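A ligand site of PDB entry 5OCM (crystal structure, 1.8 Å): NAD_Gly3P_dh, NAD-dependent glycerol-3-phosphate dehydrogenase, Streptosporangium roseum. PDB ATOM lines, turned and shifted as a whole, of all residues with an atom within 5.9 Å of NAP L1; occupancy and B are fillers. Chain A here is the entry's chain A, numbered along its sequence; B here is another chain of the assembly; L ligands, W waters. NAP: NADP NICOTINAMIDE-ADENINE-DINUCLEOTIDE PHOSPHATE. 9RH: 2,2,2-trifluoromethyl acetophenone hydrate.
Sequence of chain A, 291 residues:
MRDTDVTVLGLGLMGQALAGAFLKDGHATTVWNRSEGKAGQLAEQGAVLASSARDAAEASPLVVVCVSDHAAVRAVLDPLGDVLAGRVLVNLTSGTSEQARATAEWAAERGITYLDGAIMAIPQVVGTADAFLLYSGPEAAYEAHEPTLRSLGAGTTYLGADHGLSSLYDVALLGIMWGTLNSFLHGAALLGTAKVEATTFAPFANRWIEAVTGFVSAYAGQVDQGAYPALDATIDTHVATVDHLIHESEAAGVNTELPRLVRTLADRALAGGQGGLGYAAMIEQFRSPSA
Water W7 lies within hydrogen-bond range of O2N of NAP L1 (2.6 Å), N of Gly 12 (2.9 Å), N of Gly 15 (2.9 Å) and O of Cys 66 (3.0 Å). Water W6 bridges O2D of NAP L1 (2.7 Å) and O of Thr 237 of chain B (2.9 Å). Water W3 lies within hydrogen-bond range of OG1 of Thr 237 of chain B (2.8 Å), O1N of NAP L1 (2.9 Å) and N of Thr 234 of chain B (3.2 Å). Water W8 lies within hydrogen-bond range of the side-chain amide oxygen (OD1) of Asn 33 (2.8 Å), the backbone NH (N) of Arg 34 (2.9 Å) and a nitrogen (N3A) of NAP L1 (3.0 Å).
The side-chain hydroxyl (OG1) of Thr 237 of chain B sits at hydrogen-bond distance from the side-chain hydroxyl (OG1) of Thr 234 of chain B (3.0 Å). The side-chain amide oxygen (OD1) of Asn 33 sits at hydrogen-bond distance from the backbone NH (N) of Leu 11 (2.9 Å). N of Val 67 lies within hydrogen-bond range of OG1 of Thr 93. N of Gly 10 is in hydrogen-bond range of O of Trp 32 (2.9 Å). The backbone NH (N) of Ala 72 is in hydrogen-bond range of the side-chain carboxylate (OD1) of Asp 69. The backbone carbonyl oxygen (O) of Ser 35 sits at hydrogen-bond distance from the side-chain amide nitrogen (ND2) of Asn 33, 2.9 Å away.
O3X of NAP L1 lies within salt-bridge range of NH1 of Arg 34 (2.9 Å). OG1 of Thr 241 of chain B is in hydrogen-bond range of O2 of 9RH L2, at 2.8 Å. An oxygen (O2D) of NAP L1 sits at hydrogen-bond distance from the side-chain hydroxyl of Ser 94 (2.6 Å). An oxygen (O3B) of NAP L1 lies within hydrogen-bond range of the side-chain amide oxygen of Asn 33. O3B of NAP L1 lies within hydrogen-bond range of N of Gly 12, 3.2 Å away. The backbone NH (N) of Ser 35 sits at hydrogen-bond distance from an oxygen (O2X) of NAP L1, 3.1 Å away. An oxygen (O3B) of NAP L1 is in hydrogen-bond range of the backbone NH (N) of Leu 11, at 3.3 Å. The backbone NH of Ser 94 sits at hydrogen-bond distance from an oxygen (O3D) of NAP L1, at 3.0 Å. O2X of NAP L1 is in hydrogen-bond range of OG of Ser 35, at 2.6 Å. The backbone carbonyl oxygen (O) of Asp 232 of chain B is in hydrogen-bond range of a nitrogen (N7N) of NAP L1 (2.8 Å). O of Ser 68 is in hydrogen-bond range of O3D of NAP L1. O1A of NAP L1 sits at hydrogen-bond distance from N of Leu 13, at 3.1 Å. An oxygen (O4D) of NAP L1 sits at hydrogen-bond distance from the side-chain sulfur of Cys 66 (3.4 Å). The backbone NH (N) of Met 14 sits at hydrogen-bond distance from an oxygen (O2N) of NAP L1. An oxygen (O3D) of NAP L1 sits at hydrogen-bond distance from the backbone carbonyl oxygen of Val 67 (3.0 Å). O4B of NAP L1 is in hydrogen-bond range of N of Ser 68 (3.1 Å).
Merely in contact with NAP L1: Gly 10 (3.8 Å), Gly 15 (3.95 Å), Ala 72 (3.5 Å), Val 76 (3.4 Å), Thr 93 (3.8 Å), Ile 119 (3.4 Å), Ala 121 (3.3 Å), Ile 122 (3.9 Å), Pro 123 (3.2 Å), Ala 233 of chain B (3.6 Å), Thr 237 of chain B (3.8 Å) and Thr 241 of chain B (3.9 Å). Hydrophobic or aromatic side chains that line NAP L1: Leu 13, Met 14, Val 67, Ala 72, Val 76, Pro 123 and Ala 233 of chain B. 24 residues have an atom within 4 Å of NAP L1: Gly 10, Leu 11, Gly 12, Leu 13, Met 14, Gly 15, Asn 33, Arg 34, Ser 35, Cys 66, Val 67, Ser 68, Ala 72, Val 76, Thr 93, Ser 94, Ile 119, Ala 121, Ile 122, Pro 123, Asp 232 of chain B, Ala 233 of chain B, Thr 237 of chain B and Thr 241 of chain B. The nearest printed residue that does not touch NAP L1 is Ala 75 (4.1 Å).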
ATOM      1  N   GLY A  10     -18.005 -23.178  16.356  1.00  0.00           N
ATOM      2  CA  GLY A  10     -16.717 -23.784  16.648  1.00  0.00           C
ATOM      3  C   GLY A  10     -16.397 -23.636  18.115  1.00  0.00           C
ATOM      4  O   GLY A  10     -16.238 -22.522  18.610  1.00  0.00           O
ATOM      5  N   LEU A  11     -16.357 -24.762  18.818  1.00  0.00           N
ATOM      6  CA  LEU A  11     -16.166 -24.796  20.260  1.00  0.00           C
ATOM      7  C   LEU A  11     -14.956 -25.619  20.640  1.00  0.00           C
ATOM      8  O   LEU A  11     -15.012 -26.447  21.558  1.00  0.00           O
ATOM      9  CB  LEU A  11     -17.411 -25.318  20.958  1.00  0.00           C
ATOM     10  CG  LEU A  11     -18.657 -24.518  20.733  1.00  0.00           C
ATOM     11  CD1 LEU A  11     -19.843 -25.187  21.453  1.00  0.00           C
ATOM     12  CD2 LEU A  11     -18.551 -23.028  21.118  1.00  0.00           C
ATOM     13  N   GLY A  12     -13.851 -25.313  19.991  1.00  0.00           N
ATOM     14  CA  GLY A  12     -12.524 -25.774  20.452  1.00  0.00           C
ATOM     15  C   GLY A  12     -12.089 -25.002  21.655  1.00  0.00           C
ATOM     16  O   GLY A  12     -12.871 -24.296  22.296  1.00  0.00           O
ATOM     17  N   LEU A  13     -10.805 -25.118  22.017  1.00  0.00           N
ATOM     18  CA  LEU A  13     -10.283 -24.372  23.166  1.00  0.00           C
ATOM     19  C   LEU A  13     -10.568 -22.883  22.999  1.00  0.00           C
ATOM     20  O   LEU A  13     -10.940 -22.196  23.947  1.00  0.00           O
ATOM     21  CB  LEU A  13      -8.752 -24.553  23.263  1.00  0.00           C
ATOM     22  CG  LEU A  13      -8.281 -25.951  23.567  1.00  0.00           C
ATOM     23  CD1 LEU A  13      -6.767 -25.921  23.749  1.00  0.00           C
ATOM     24  CD2 LEU A  13      -8.880 -26.530  24.861  1.00  0.00           C
ATOM     25  N   MET A  14     -10.413 -22.362  21.786  1.00  0.00           N
ATOM     26  CA  MET A  14     -10.598 -20.942  21.596  1.00  0.00           C
ATOM     27  C   MET A  14     -12.073 -20.547  21.474  1.00  0.00           C
ATOM     28  O   MET A  14     -12.538 -19.585  22.087  1.00  0.00           O
ATOM     29  CB  MET A  14      -9.770 -20.434  20.410  1.00  0.00           C
ATOM     30  CG  MET A  14      -9.908 -18.952  20.178  1.00  0.00           C
ATOM     31  SD  MET A  14      -9.595 -17.817  21.587  1.00  0.00           S
ATOM     32  CE  MET A  14      -7.801 -17.930  21.562  1.00  0.00           C
ATOM     33  N   GLY A  15     -12.818 -21.286  20.656  1.00  0.00           N
ATOM     34  CA  GLY A  15     -14.262 -21.029  20.571  1.00  0.00           C
ATOM     35  C   GLY A  15     -14.965 -21.054  21.892  1.00  0.00           C
ATOM     36  O   GLY A  15     -15.867 -20.253  22.139  1.00  0.00           O
ATOM     37  N   TRP A  32     -22.636 -23.591  18.646  1.00  0.00           N
ATOM     38  CA  TRP A  32     -22.711 -24.831  17.889  1.00  0.00           C
ATOM     39  C   TRP A  32     -21.302 -25.321  17.641  1.00  0.00           C
ATOM     40  O   TRP A  32     -20.359 -24.531  17.452  1.00  0.00           O
ATOM     41  CB  TRP A  32     -23.424 -24.635  16.541  1.00  0.00           C
ATOM     42  CG  TRP A  32     -23.352 -25.851  15.658  1.00  0.00           C
ATOM     43  CD1 TRP A  32     -24.180 -26.960  15.665  1.00  0.00           C
ATOM     44  CD2 TRP A  32     -22.369 -26.130  14.652  1.00  0.00           C
ATOM     45  NE1 TRP A  32     -23.792 -27.873  14.741  1.00  0.00           N
ATOM     46  CE2 TRP A  32     -22.676 -27.404  14.099  1.00  0.00           C
ATOM     47  CE3 TRP A  32     -21.248 -25.445  14.196  1.00  0.00           C
ATOM     48  CZ2 TRP A  32     -21.914 -27.983  13.082  1.00  0.00           C
ATOM     49  CZ3 TRP A  32     -20.480 -26.041  13.163  1.00  0.00           C
ATOM     50  CH2 TRP A  32     -20.830 -27.273  12.625  1.00  0.00           C
ATOM     51  N   ASN A  33     -21.148 -26.642  17.611  1.00  0.00           N
ATOM     52  CA  ASN A  33     -19.888 -27.329  17.277  1.00  0.00           C
ATOM     53  C   ASN A  33     -20.223 -28.557  16.457  1.00  0.00           C
ATOM     54  O   ASN A  33     -21.263 -29.192  16.710  1.00  0.00           O
ATOM     55  CB  ASN A  33     -19.175 -27.761  18.542  1.00  0.00           C
ATOM     56  CG  ASN A  33     -17.734 -28.189  18.272  1.00  0.00           C
ATOM     57  OD1 ASN A  33     -16.933 -27.384  17.703  1.00  0.00           O
ATOM     58  ND2 ASN A  33     -17.400 -29.468  18.616  1.00  0.00           N
ATOM     59  N   ARG A  34     -19.361 -28.918  15.531  1.00  0.00           N
ATOM     60  CA  ARG A  34     -19.573 -30.156  14.722  1.00  0.00           C
ATOM     61  C   ARG A  34     -19.793 -31.360  15.588  1.00  0.00           C
ATOM     62  O   ARG A  34     -20.729 -32.091  15.366  1.00  0.00           O
ATOM     63  CB  ARG A  34     -18.353 -30.358  13.796  1.00  0.00           C
ATOM     64  CG  ARG A  34     -18.277 -31.737  13.165  1.00  0.00           C
ATOM     65  CD  ARG A  34     -17.087 -31.798  12.248  1.00  0.00           C
ATOM     66  NE  ARG A  34     -15.829 -31.770  12.973  1.00  0.00           N
ATOM     67  CZ  ARG A  34     -14.644 -31.955  12.409  1.00  0.00           C
ATOM     68  NH1 ARG A  34     -13.546 -31.916  13.150  1.00  0.00           N
ATOM     69  NH2 ARG A  34     -14.525 -32.202  11.096  1.00  0.00           N
ATOM     70  N   SER A  35     -18.921 -31.573  16.553  1.00  0.00           N
ATOM     71  CA  SER A  35     -19.030 -32.688  17.500  1.00  0.00           C
ATOM     72  C   SER A  35     -19.833 -32.318  18.725  1.00  0.00           C
ATOM     73  O   SER A  35     -19.588 -31.288  19.332  1.00  0.00           O
ATOM     74  CB  SER A  35     -17.631 -33.112  17.970  1.00  0.00           C
ATOM     75  OG  SER A  35     -16.876 -33.536  16.867  1.00  0.00           O
ATOM     76  N   LYS A  38     -19.203 -30.746  23.649  1.00  0.00           N
ATOM     77  CA  LYS A  38     -18.154 -29.776  24.028  1.00  0.00           C
ATOM     78  C   LYS A  38     -18.777 -28.555  24.752  1.00  0.00           C
ATOM     79  O   LYS A  38     -18.067 -27.622  25.015  1.00  0.00           O
ATOM     80  CB  LYS A  38     -17.356 -29.341  22.740  1.00  0.00           C
ATOM     81  CG  LYS A  38     -16.255 -30.352  22.297  1.00  0.00           C
ATOM     82  CD  LYS A  38     -16.617 -31.760  21.861  1.00  0.00           C
ATOM     83  N   CYS A  66     -14.930 -19.763  14.532  1.00  0.00           N
ATOM     84  CA  CYS A  66     -13.548 -20.018  15.022  1.00  0.00           C
ATOM     85  C   CYS A  66     -13.303 -21.509  14.983  1.00  0.00           C
ATOM     86  O   CYS A  66     -13.533 -22.217  15.946  1.00  0.00           O
ATOM     87  CB  CYS A  66     -13.345 -19.429  16.377  1.00  0.00           C
ATOM     88  SG  CYS A  66     -11.605 -19.555  16.927  1.00  0.00           S
ATOM     89  N   VAL A  67     -12.939 -21.983  13.784  1.00  0.00           N
ATOM     90  CA  VAL A  67     -12.657 -23.418  13.552  1.00  0.00           C
ATOM     91  C   VAL A  67     -11.181 -23.586  13.210  1.00  0.00           C
ATOM     92  O   VAL A  67     -10.383 -22.645  13.403  1.00  0.00           O
ATOM     93  CB  VAL A  67     -13.635 -24.054  12.535  1.00  0.00           C
ATOM     94  CG1 VAL A  67     -15.045 -24.053  13.125  1.00  0.00           C
ATOM     95  CG2 VAL A  67     -13.582 -23.321  11.166  1.00  0.00           C
ATOM     96  N   SER A  68     -10.763 -24.766  12.783  1.00  0.00           N
ATOM     97  CA  SER A  68      -9.327 -25.035  12.659  1.00  0.00           C
ATOM     98  C   SER A  68      -8.659 -24.200  11.522  1.00  0.00           C
ATOM     99  O   SER A  68      -7.724 -23.454  11.770  1.00  0.00           O
ATOM    100  CB  SER A  68      -9.098 -26.540  12.470  1.00  0.00           C
ATOM    101  OG  SER A  68      -9.881 -26.920  11.310  1.00  0.00           O
ATOM    102  N   ASP A  69      -9.184 -24.297  10.320  1.00  0.00           N
ATOM    103  CA  ASP A  69      -8.538 -23.666   9.161  1.00  0.00           C
ATOM    104  C   ASP A  69      -9.559 -23.326   8.088  1.00  0.00           C
ATOM    105  O   ASP A  69     -10.732 -23.566   8.259  1.00  0.00           O
ATOM    106  CB  ASP A  69      -7.425 -24.597   8.618  1.00  0.00           C
ATOM    107  CG  ASP A  69      -7.967 -25.948   8.151  1.00  0.00           C
ATOM    108  OD1 ASP A  69      -9.210 -26.154   7.882  1.00  0.00           O
ATOM    109  OD2 ASP A  69      -7.111 -26.824   7.941  1.00  0.00           O
ATOM    110  N   ALA A  71     -10.248 -24.573   5.187  1.00  0.00           N
ATOM    111  CA  ALA A  71     -11.047 -25.698   4.657  1.00  0.00           C
ATOM    112  C   ALA A  71     -12.281 -25.970   5.557  1.00  0.00           C
ATOM    113  O   ALA A  71     -13.387 -26.167   5.042  1.00  0.00           O
ATOM    114  CB  ALA A  71     -10.214 -26.963   4.510  1.00  0.00           C
ATOM    115  N   ALA A  72     -12.081 -25.937   6.865  1.00  0.00           N
ATOM    116  CA  ALA A  72     -13.171 -26.025   7.808  1.00  0.00           C
ATOM    117  C   ALA A  72     -14.157 -24.892   7.738  1.00  0.00           C
ATOM    118  O   ALA A  72     -15.400 -25.097   7.769  1.00  0.00           O
ATOM    119  CB  ALA A  72     -12.632 -26.195   9.247  1.00  0.00           C
ATOM    120  N   ALA A  75     -16.299 -25.493   4.726  1.00  0.00           N
ATOM    121  CA  ALA A  75     -17.228 -26.573   5.016  1.00  0.00           C
ATOM    122  C   ALA A  75     -18.430 -26.064   5.854  1.00  0.00           C
ATOM    123  O   ALA A  75     -19.568 -26.461   5.577  1.00  0.00           O
ATOM    124  CB  ALA A  75     -16.536 -27.721   5.742  1.00  0.00           C
ATOM    125  N   VAL A  76     -18.187 -25.218   6.845  1.00  0.00           N
ATOM    126  CA  VAL A  76     -19.262 -24.720   7.704  1.00  0.00           C
ATOM    127  C   VAL A  76     -20.108 -23.700   6.962  1.00  0.00           C
ATOM    128  O   VAL A  76     -21.345 -23.724   7.039  1.00  0.00           O
ATOM    129  CB  VAL A  76     -18.703 -24.154   9.021  1.00  0.00           C
ATOM    130  CG1 VAL A  76     -19.790 -23.451   9.794  1.00  0.00           C
ATOM    131  CG2 VAL A  76     -18.104 -25.267   9.873  1.00  0.00           C
ATOM    132  N   LEU A  92     -12.701 -15.576  12.758  1.00  0.00           N
ATOM    133  CA  LEU A  92     -11.524 -15.518  13.635  1.00  0.00           C
ATOM    134  C   LEU A  92     -10.644 -16.755  13.485  1.00  0.00           C
ATOM    135  O   LEU A  92      -9.727 -17.034  14.306  1.00  0.00           O
ATOM    136  CB  LEU A  92     -11.950 -15.307  15.096  1.00  0.00           C
ATOM    137  CG  LEU A  92     -12.722 -14.009  15.401  1.00  0.00           C
ATOM    138  CD1 LEU A  92     -13.083 -13.902  16.867  1.00  0.00           C
ATOM    139  CD2 LEU A  92     -11.962 -12.811  14.887  1.00  0.00           C
ATOM    140  N   THR A  93     -10.896 -17.551  12.442  1.00  0.00           N
ATOM    141  CA  THR A  93     -10.070 -18.727  12.150  1.00  0.00           C
ATOM    142  C   THR A  93      -8.702 -18.289  11.580  1.00  0.00           C
ATOM    143  O   THR A  93      -8.657 -17.410  10.767  1.00  0.00           O
ATOM    144  CB  THR A  93     -10.820 -19.601  11.117  1.00  0.00           C
ATOM    145  OG1 THR A  93     -12.116 -19.932  11.678  1.00  0.00           O
ATOM    146  CG2 THR A  93     -10.072 -20.848  10.800  1.00  0.00           C
ATOM    147  N   SER A  94      -7.616 -18.943  11.983  1.00  0.00           N
ATOM    148  CA  SER A  94      -6.294 -18.679  11.408  1.00  0.00           C
ATOM    149  C   SER A  94      -6.242 -19.004   9.909  1.00  0.00           C
ATOM    150  O   SER A  94      -6.921 -19.881   9.423  1.00  0.00           O
ATOM    151  CB  SER A  94      -5.208 -19.451  12.142  1.00  0.00           C
ATOM    152  OG  SER A  94      -5.280 -19.220  13.509  1.00  0.00           O
ATOM    153  N   GLY A  95      -5.396 -18.265   9.196  1.00  0.00           N
ATOM    154  CA  GLY A  95      -5.186 -18.558   7.768  1.00  0.00           C
ATOM    155  C   GLY A  95      -4.291 -17.534   7.115  1.00  0.00           C
ATOM    156  O   GLY A  95      -3.671 -16.721   7.814  1.00  0.00           O
ATOM    157  N   ILE A 119      -7.058 -13.375  16.437  1.00  0.00           N
ATOM    158  CA  ILE A 119      -7.068 -13.371  17.885  1.00  0.00           C
ATOM    159  C   ILE A 119      -5.639 -13.417  18.365  1.00  0.00           C
ATOM    160  O   ILE A 119      -4.999 -14.478  18.266  1.00  0.00           O
ATOM    161  CB  ILE A 119      -7.828 -14.549  18.491  1.00  0.00           C
ATOM    162  CG1 ILE A 119      -9.268 -14.611  17.938  1.00  0.00           C
ATOM    163  CG2 ILE A 119      -7.924 -14.396  20.030  1.00  0.00           C
ATOM    164  CD1 ILE A 119      -9.884 -16.017  18.114  1.00  0.00           C
ATOM    165  N   MET A 120      -5.132 -12.280  18.869  1.00  0.00           N
ATOM    166  CA  MET A 120      -3.739 -12.220  19.320  1.00  0.00           C
ATOM    167  C   MET A 120      -3.741 -12.396  20.838  1.00  0.00           C
ATOM    168  O   MET A 120      -3.373 -11.507  21.595  1.00  0.00           O
ATOM    169  CB  MET A 120      -3.074 -10.904  18.894  1.00  0.00           C
ATOM    170  CG  MET A 120      -3.158 -10.608  17.405  1.00  0.00           C
ATOM    171  SD  MET A 120      -2.827 -11.946  16.252  1.00  0.00           S
ATOM    172  CE  MET A 120      -1.209 -12.472  16.827  1.00  0.00           C
ATOM    173  N   ALA A 121      -4.199 -13.563  21.250  1.00  0.00           N
ATOM    174  CA  ALA A 121      -4.401 -13.930  22.637  1.00  0.00           C
ATOM    175  C   ALA A 121      -4.607 -15.408  22.764  1.00  0.00           C
ATOM    176  O   ALA A 121      -5.054 -16.066  21.822  1.00  0.00           O
ATOM    177  CB  ALA A 121      -5.656 -13.205  23.188  1.00  0.00           C
ATOM    178  N   ILE A 122      -4.324 -15.908  23.957  1.00  0.00           N
ATOM    179  CA  ILE A 122      -4.684 -17.277  24.317  1.00  0.00           C
ATOM    180  C   ILE A 122      -6.104 -17.314  24.959  1.00  0.00           C
ATOM    181  O   ILE A 122      -6.618 -16.285  25.407  1.00  0.00           O
ATOM    182  CB  ILE A 122      -3.653 -17.921  25.290  1.00  0.00           C
ATOM    183  CG1 ILE A 122      -3.466 -17.052  26.554  1.00  0.00           C
ATOM    184  CG2 ILE A 122      -2.353 -18.173  24.562  1.00  0.00           C
ATOM    185  CD1 ILE A 122      -2.645 -17.725  27.668  1.00  0.00           C
ATOM    186  N   PRO A 123      -6.701 -18.502  25.016  1.00  0.00           N
ATOM    187  CA  PRO A 123      -8.103 -18.565  25.489  1.00  0.00           C
ATOM    188  C   PRO A 123      -8.328 -17.989  26.872  1.00  0.00           C
ATOM    189  O   PRO A 123      -9.323 -17.320  27.098  1.00  0.00           O
ATOM    190  CB  PRO A 123      -8.394 -20.072  25.458  1.00  0.00           C
ATOM    191  CG  PRO A 123      -7.552 -20.590  24.364  1.00  0.00           C
ATOM    192  CD  PRO A 123      -6.243 -19.834  24.541  1.00  0.00           C
ATOM    193  N   ASP B 232      -3.730 -23.828  26.516  1.00  0.00           N
ATOM    194  CA  ASP B 232      -4.019 -22.738  25.570  1.00  0.00           C
ATOM    195  C   ASP B 232      -4.166 -23.237  24.154  1.00  0.00           C
ATOM    196  O   ASP B 232      -5.233 -23.044  23.558  1.00  0.00           O
ATOM    197  CB  ASP B 232      -2.985 -21.574  25.684  1.00  0.00           C
ATOM    198  CG  ASP B 232      -1.544 -22.019  25.810  1.00  0.00           C
ATOM    199  OD1 ASP B 232      -1.213 -23.212  25.552  1.00  0.00           O
ATOM    200  OD2 ASP B 232      -0.735 -21.097  26.139  1.00  0.00           O
ATOM    201  N   ALA B 233      -3.139 -23.869  23.610  1.00  0.00           N
ATOM    202  CA  ALA B 233      -3.098 -24.357  22.248  1.00  0.00           C
ATOM    203  C   ALA B 233      -2.173 -25.571  22.149  1.00  0.00           C
ATOM    204  O   ALA B 233      -1.149 -25.599  22.798  1.00  0.00           O
ATOM    205  CB  ALA B 233      -2.560 -23.274  21.307  1.00  0.00           C
ATOM    206  N   THR B 234      -2.550 -26.556  21.332  1.00  0.00           N
ATOM    207  CA  THR B 234      -1.676 -27.722  21.110  1.00  0.00           C
ATOM    208  C   THR B 234      -0.562 -27.391  20.096  1.00  0.00           C
ATOM    209  O   THR B 234      -0.681 -26.454  19.232  1.00  0.00           O
ATOM    210  CB  THR B 234      -2.482 -28.907  20.525  1.00  0.00           C
ATOM    211  OG1 THR B 234      -3.044 -28.514  19.264  1.00  0.00           O
ATOM    212  CG2 THR B 234      -3.606 -29.320  21.482  1.00  0.00           C
ATOM    213  N   THR B 237      -1.936 -27.370  16.657  1.00  0.00           N
ATOM    214  CA  THR B 237      -2.569 -26.087  16.288  1.00  0.00           C
ATOM    215  C   THR B 237      -1.482 -25.048  15.899  1.00  0.00           C
ATOM    216  O   THR B 237      -1.595 -24.334  14.876  1.00  0.00           O
ATOM    217  CB  THR B 237      -3.454 -25.609  17.426  1.00  0.00           C
ATOM    218  OG1 THR B 237      -4.510 -26.554  17.589  1.00  0.00           O
ATOM    219  CG2 THR B 237      -4.007 -24.234  17.219  1.00  0.00           C
ATOM    220  N   THR B 241      -0.455 -22.958  11.970  1.00  0.00           N
ATOM    221  CA  THR B 241      -0.137 -21.548  11.770  1.00  0.00           C
ATOM    222  C   THR B 241       1.299 -21.303  11.297  1.00  0.00           C
ATOM    223  O   THR B 241       1.553 -20.350  10.586  1.00  0.00           O
ATOM    224  CB  THR B 241      -0.478 -20.619  12.987  1.00  0.00           C
ATOM    225  OG1 THR B 241      -0.025 -21.220  14.197  1.00  0.00           O
ATOM    226  CG2 THR B 241      -1.944 -20.431  13.063  1.00  0.00           C
HETATM  227  PA  NAP L   1      -9.194 -26.704  18.392  1.00  0.00           P
HETATM  228  O1A NAP L   1      -9.295 -26.898  19.904  1.00  0.00           O
HETATM  229  O2A NAP L   1      -8.397 -27.765  17.792  1.00  0.00           O
HETATM  230  O5B NAP L   1     -10.654 -26.584  17.674  1.00  0.00           O
HETATM  231  C5B NAP L   1     -10.778 -26.820  16.281  1.00  0.00           C
HETATM  232  C4B NAP L   1     -12.229 -26.525  16.018  1.00  0.00           C
HETATM  233  O4B NAP L   1     -12.532 -26.544  14.635  1.00  0.00           O
HETATM  234  C3B NAP L   1     -13.237 -27.507  16.706  1.00  0.00           C
HETATM  235  O3B NAP L   1     -14.416 -26.816  17.172  1.00  0.00           O
HETATM  236  C2B NAP L   1     -13.584 -28.444  15.530  1.00  0.00           C
HETATM  237  O2B NAP L   1     -14.791 -29.204  15.696  1.00  0.00           O
HETATM  238  C1B NAP L   1     -13.635 -27.455  14.393  1.00  0.00           C
HETATM  239  N9A NAP L   1     -13.522 -28.059  13.086  1.00  0.00           N
HETATM  240  C8A NAP L   1     -12.466 -28.617  12.501  1.00  0.00           C
HETATM  241  N7A NAP L   1     -12.755 -29.054  11.281  1.00  0.00           N
HETATM  242  C5A NAP L   1     -14.049 -28.762  11.082  1.00  0.00           C
HETATM  243  C6A NAP L   1     -15.000 -28.940   9.994  1.00  0.00           C
HETATM  244  N6A NAP L   1     -14.584 -29.553   8.820  1.00  0.00           N
HETATM  245  N1A NAP L   1     -16.288 -28.583  10.194  1.00  0.00           N
HETATM  246  C2A NAP L   1     -16.700 -27.999  11.337  1.00  0.00           C
HETATM  247  N3A NAP L   1     -15.880 -27.761  12.385  1.00  0.00           N
HETATM  248  C4A NAP L   1     -14.581 -28.130  12.266  1.00  0.00           C
HETATM  249  O3  NAP L   1      -8.479 -25.361  17.950  1.00  0.00           O
HETATM  250  PN  NAP L   1      -8.562 -23.960  18.798  1.00  0.00           P
HETATM  251  O1N NAP L   1      -7.359 -23.849  19.653  1.00  0.00           O
HETATM  252  O2N NAP L   1     -10.000 -23.675  19.248  1.00  0.00           O
HETATM  253  O5D NAP L   1      -8.219 -23.054  17.506  1.00  0.00           O
HETATM  254  C5D NAP L   1      -9.295 -22.634  16.661  1.00  0.00           C
HETATM  255  C4D NAP L   1      -8.748 -21.529  15.777  1.00  0.00           C
HETATM  256  O4D NAP L   1      -8.334 -20.397  16.642  1.00  0.00           O
HETATM  257  C3D NAP L   1      -7.561 -22.028  14.925  1.00  0.00           C
HETATM  258  O3D NAP L   1      -7.596 -21.425  13.612  1.00  0.00           O
HETATM  259  C2D NAP L   1      -6.388 -21.478  15.751  1.00  0.00           C
HETATM  260  O2D NAP L   1      -5.154 -21.286  15.044  1.00  0.00           O
HETATM  261  C1D NAP L   1      -6.998 -20.161  16.289  1.00  0.00           C
HETATM  262  N1N NAP L   1      -6.337 -19.649  17.474  1.00  0.00           N
HETATM  263  C2N NAP L   1      -6.239 -20.384  18.566  1.00  0.00           C
HETATM  264  C3N NAP L   1      -5.576 -19.902  19.699  1.00  0.00           C
HETATM  265  C7N NAP L   1      -5.357 -20.708  20.923  1.00  0.00           C
HETATM  266  O7N NAP L   1      -4.614 -20.181  21.787  1.00  0.00           O
HETATM  267  N7N NAP L   1      -5.909 -21.882  21.063  1.00  0.00           N
HETATM  268  C4N NAP L   1      -5.066 -18.593  19.693  1.00  0.00           C
HETATM  269  C5N NAP L   1      -5.294 -17.822  18.566  1.00  0.00           C
HETATM  270  C6N NAP L   1      -5.938 -18.385  17.474  1.00  0.00           C
HETATM  271  P2B NAP L   1     -14.746 -30.603  16.485  1.00  0.00           P
HETATM  272  O1X NAP L   1     -14.783 -30.242  17.941  1.00  0.00           O
HETATM  273  O2X NAP L   1     -15.936 -31.268  15.887  1.00  0.00           O
HETATM  274  O3X NAP L   1     -13.506 -31.317  15.942  1.00  0.00           O
HETATM  275  O1  9RH L   2      -0.865 -21.633  18.072  1.00  0.00           O
HETATM  276  C1  9RH L   2      -1.232 -20.366  17.617  1.00  0.00           C
HETATM  277  O2  9RH L   2      -0.417 -19.872  16.589  1.00  0.00           O
HETATM  278  C2  9RH L   2      -1.387 -19.386  18.765  1.00  0.00           C
HETATM  279  C3  9RH L   2      -1.054 -19.767  20.061  1.00  0.00           C
HETATM  280  C4  9RH L   2      -1.083 -18.844  21.098  1.00  0.00           C
HETATM  281  C5  9RH L   2      -1.467 -17.548  20.857  1.00  0.00           C
HETATM  282  C6  9RH L   2      -1.813 -17.168  19.587  1.00  0.00           C
HETATM  283  C7  9RH L   2      -1.769 -18.078  18.536  1.00  0.00           C
HETATM  284  C8  9RH L   2      -2.548 -20.650  16.964  1.00  0.00           C
HETATM  285  F1  9RH L   2      -2.370 -21.579  16.028  1.00  0.00           F
HETATM  286  F2  9RH L   2      -3.098 -19.532  16.425  1.00  0.00           F
HETATM  287  F3  9RH L   2      -3.333 -21.133  17.915  1.00  0.00           F
HETATM  288  O   HOH W   1     -18.319 -30.045   9.196  1.00  0.00           O
HETATM  289  O   HOH W   2      -9.766 -29.770  13.930  1.00  0.00           O
HETATM  290  O   HOH W   3      -5.450 -25.935  20.167  1.00  0.00           O
HETATM  291  O   HOH W   4     -10.934 -28.959  20.831  1.00  0.00           O
HETATM  292  O   HOH W   5      -7.064 -28.089  20.875  1.00  0.00           O
HETATM  293  O   HOH W   6      -4.074 -23.384  13.796  1.00  0.00           O
HETATM  294  O   HOH W   7     -12.498 -23.250  18.523  1.00  0.00           O
HETATM  295  O   HOH W   8     -17.213 -27.073  14.948  1.00  0.00           O
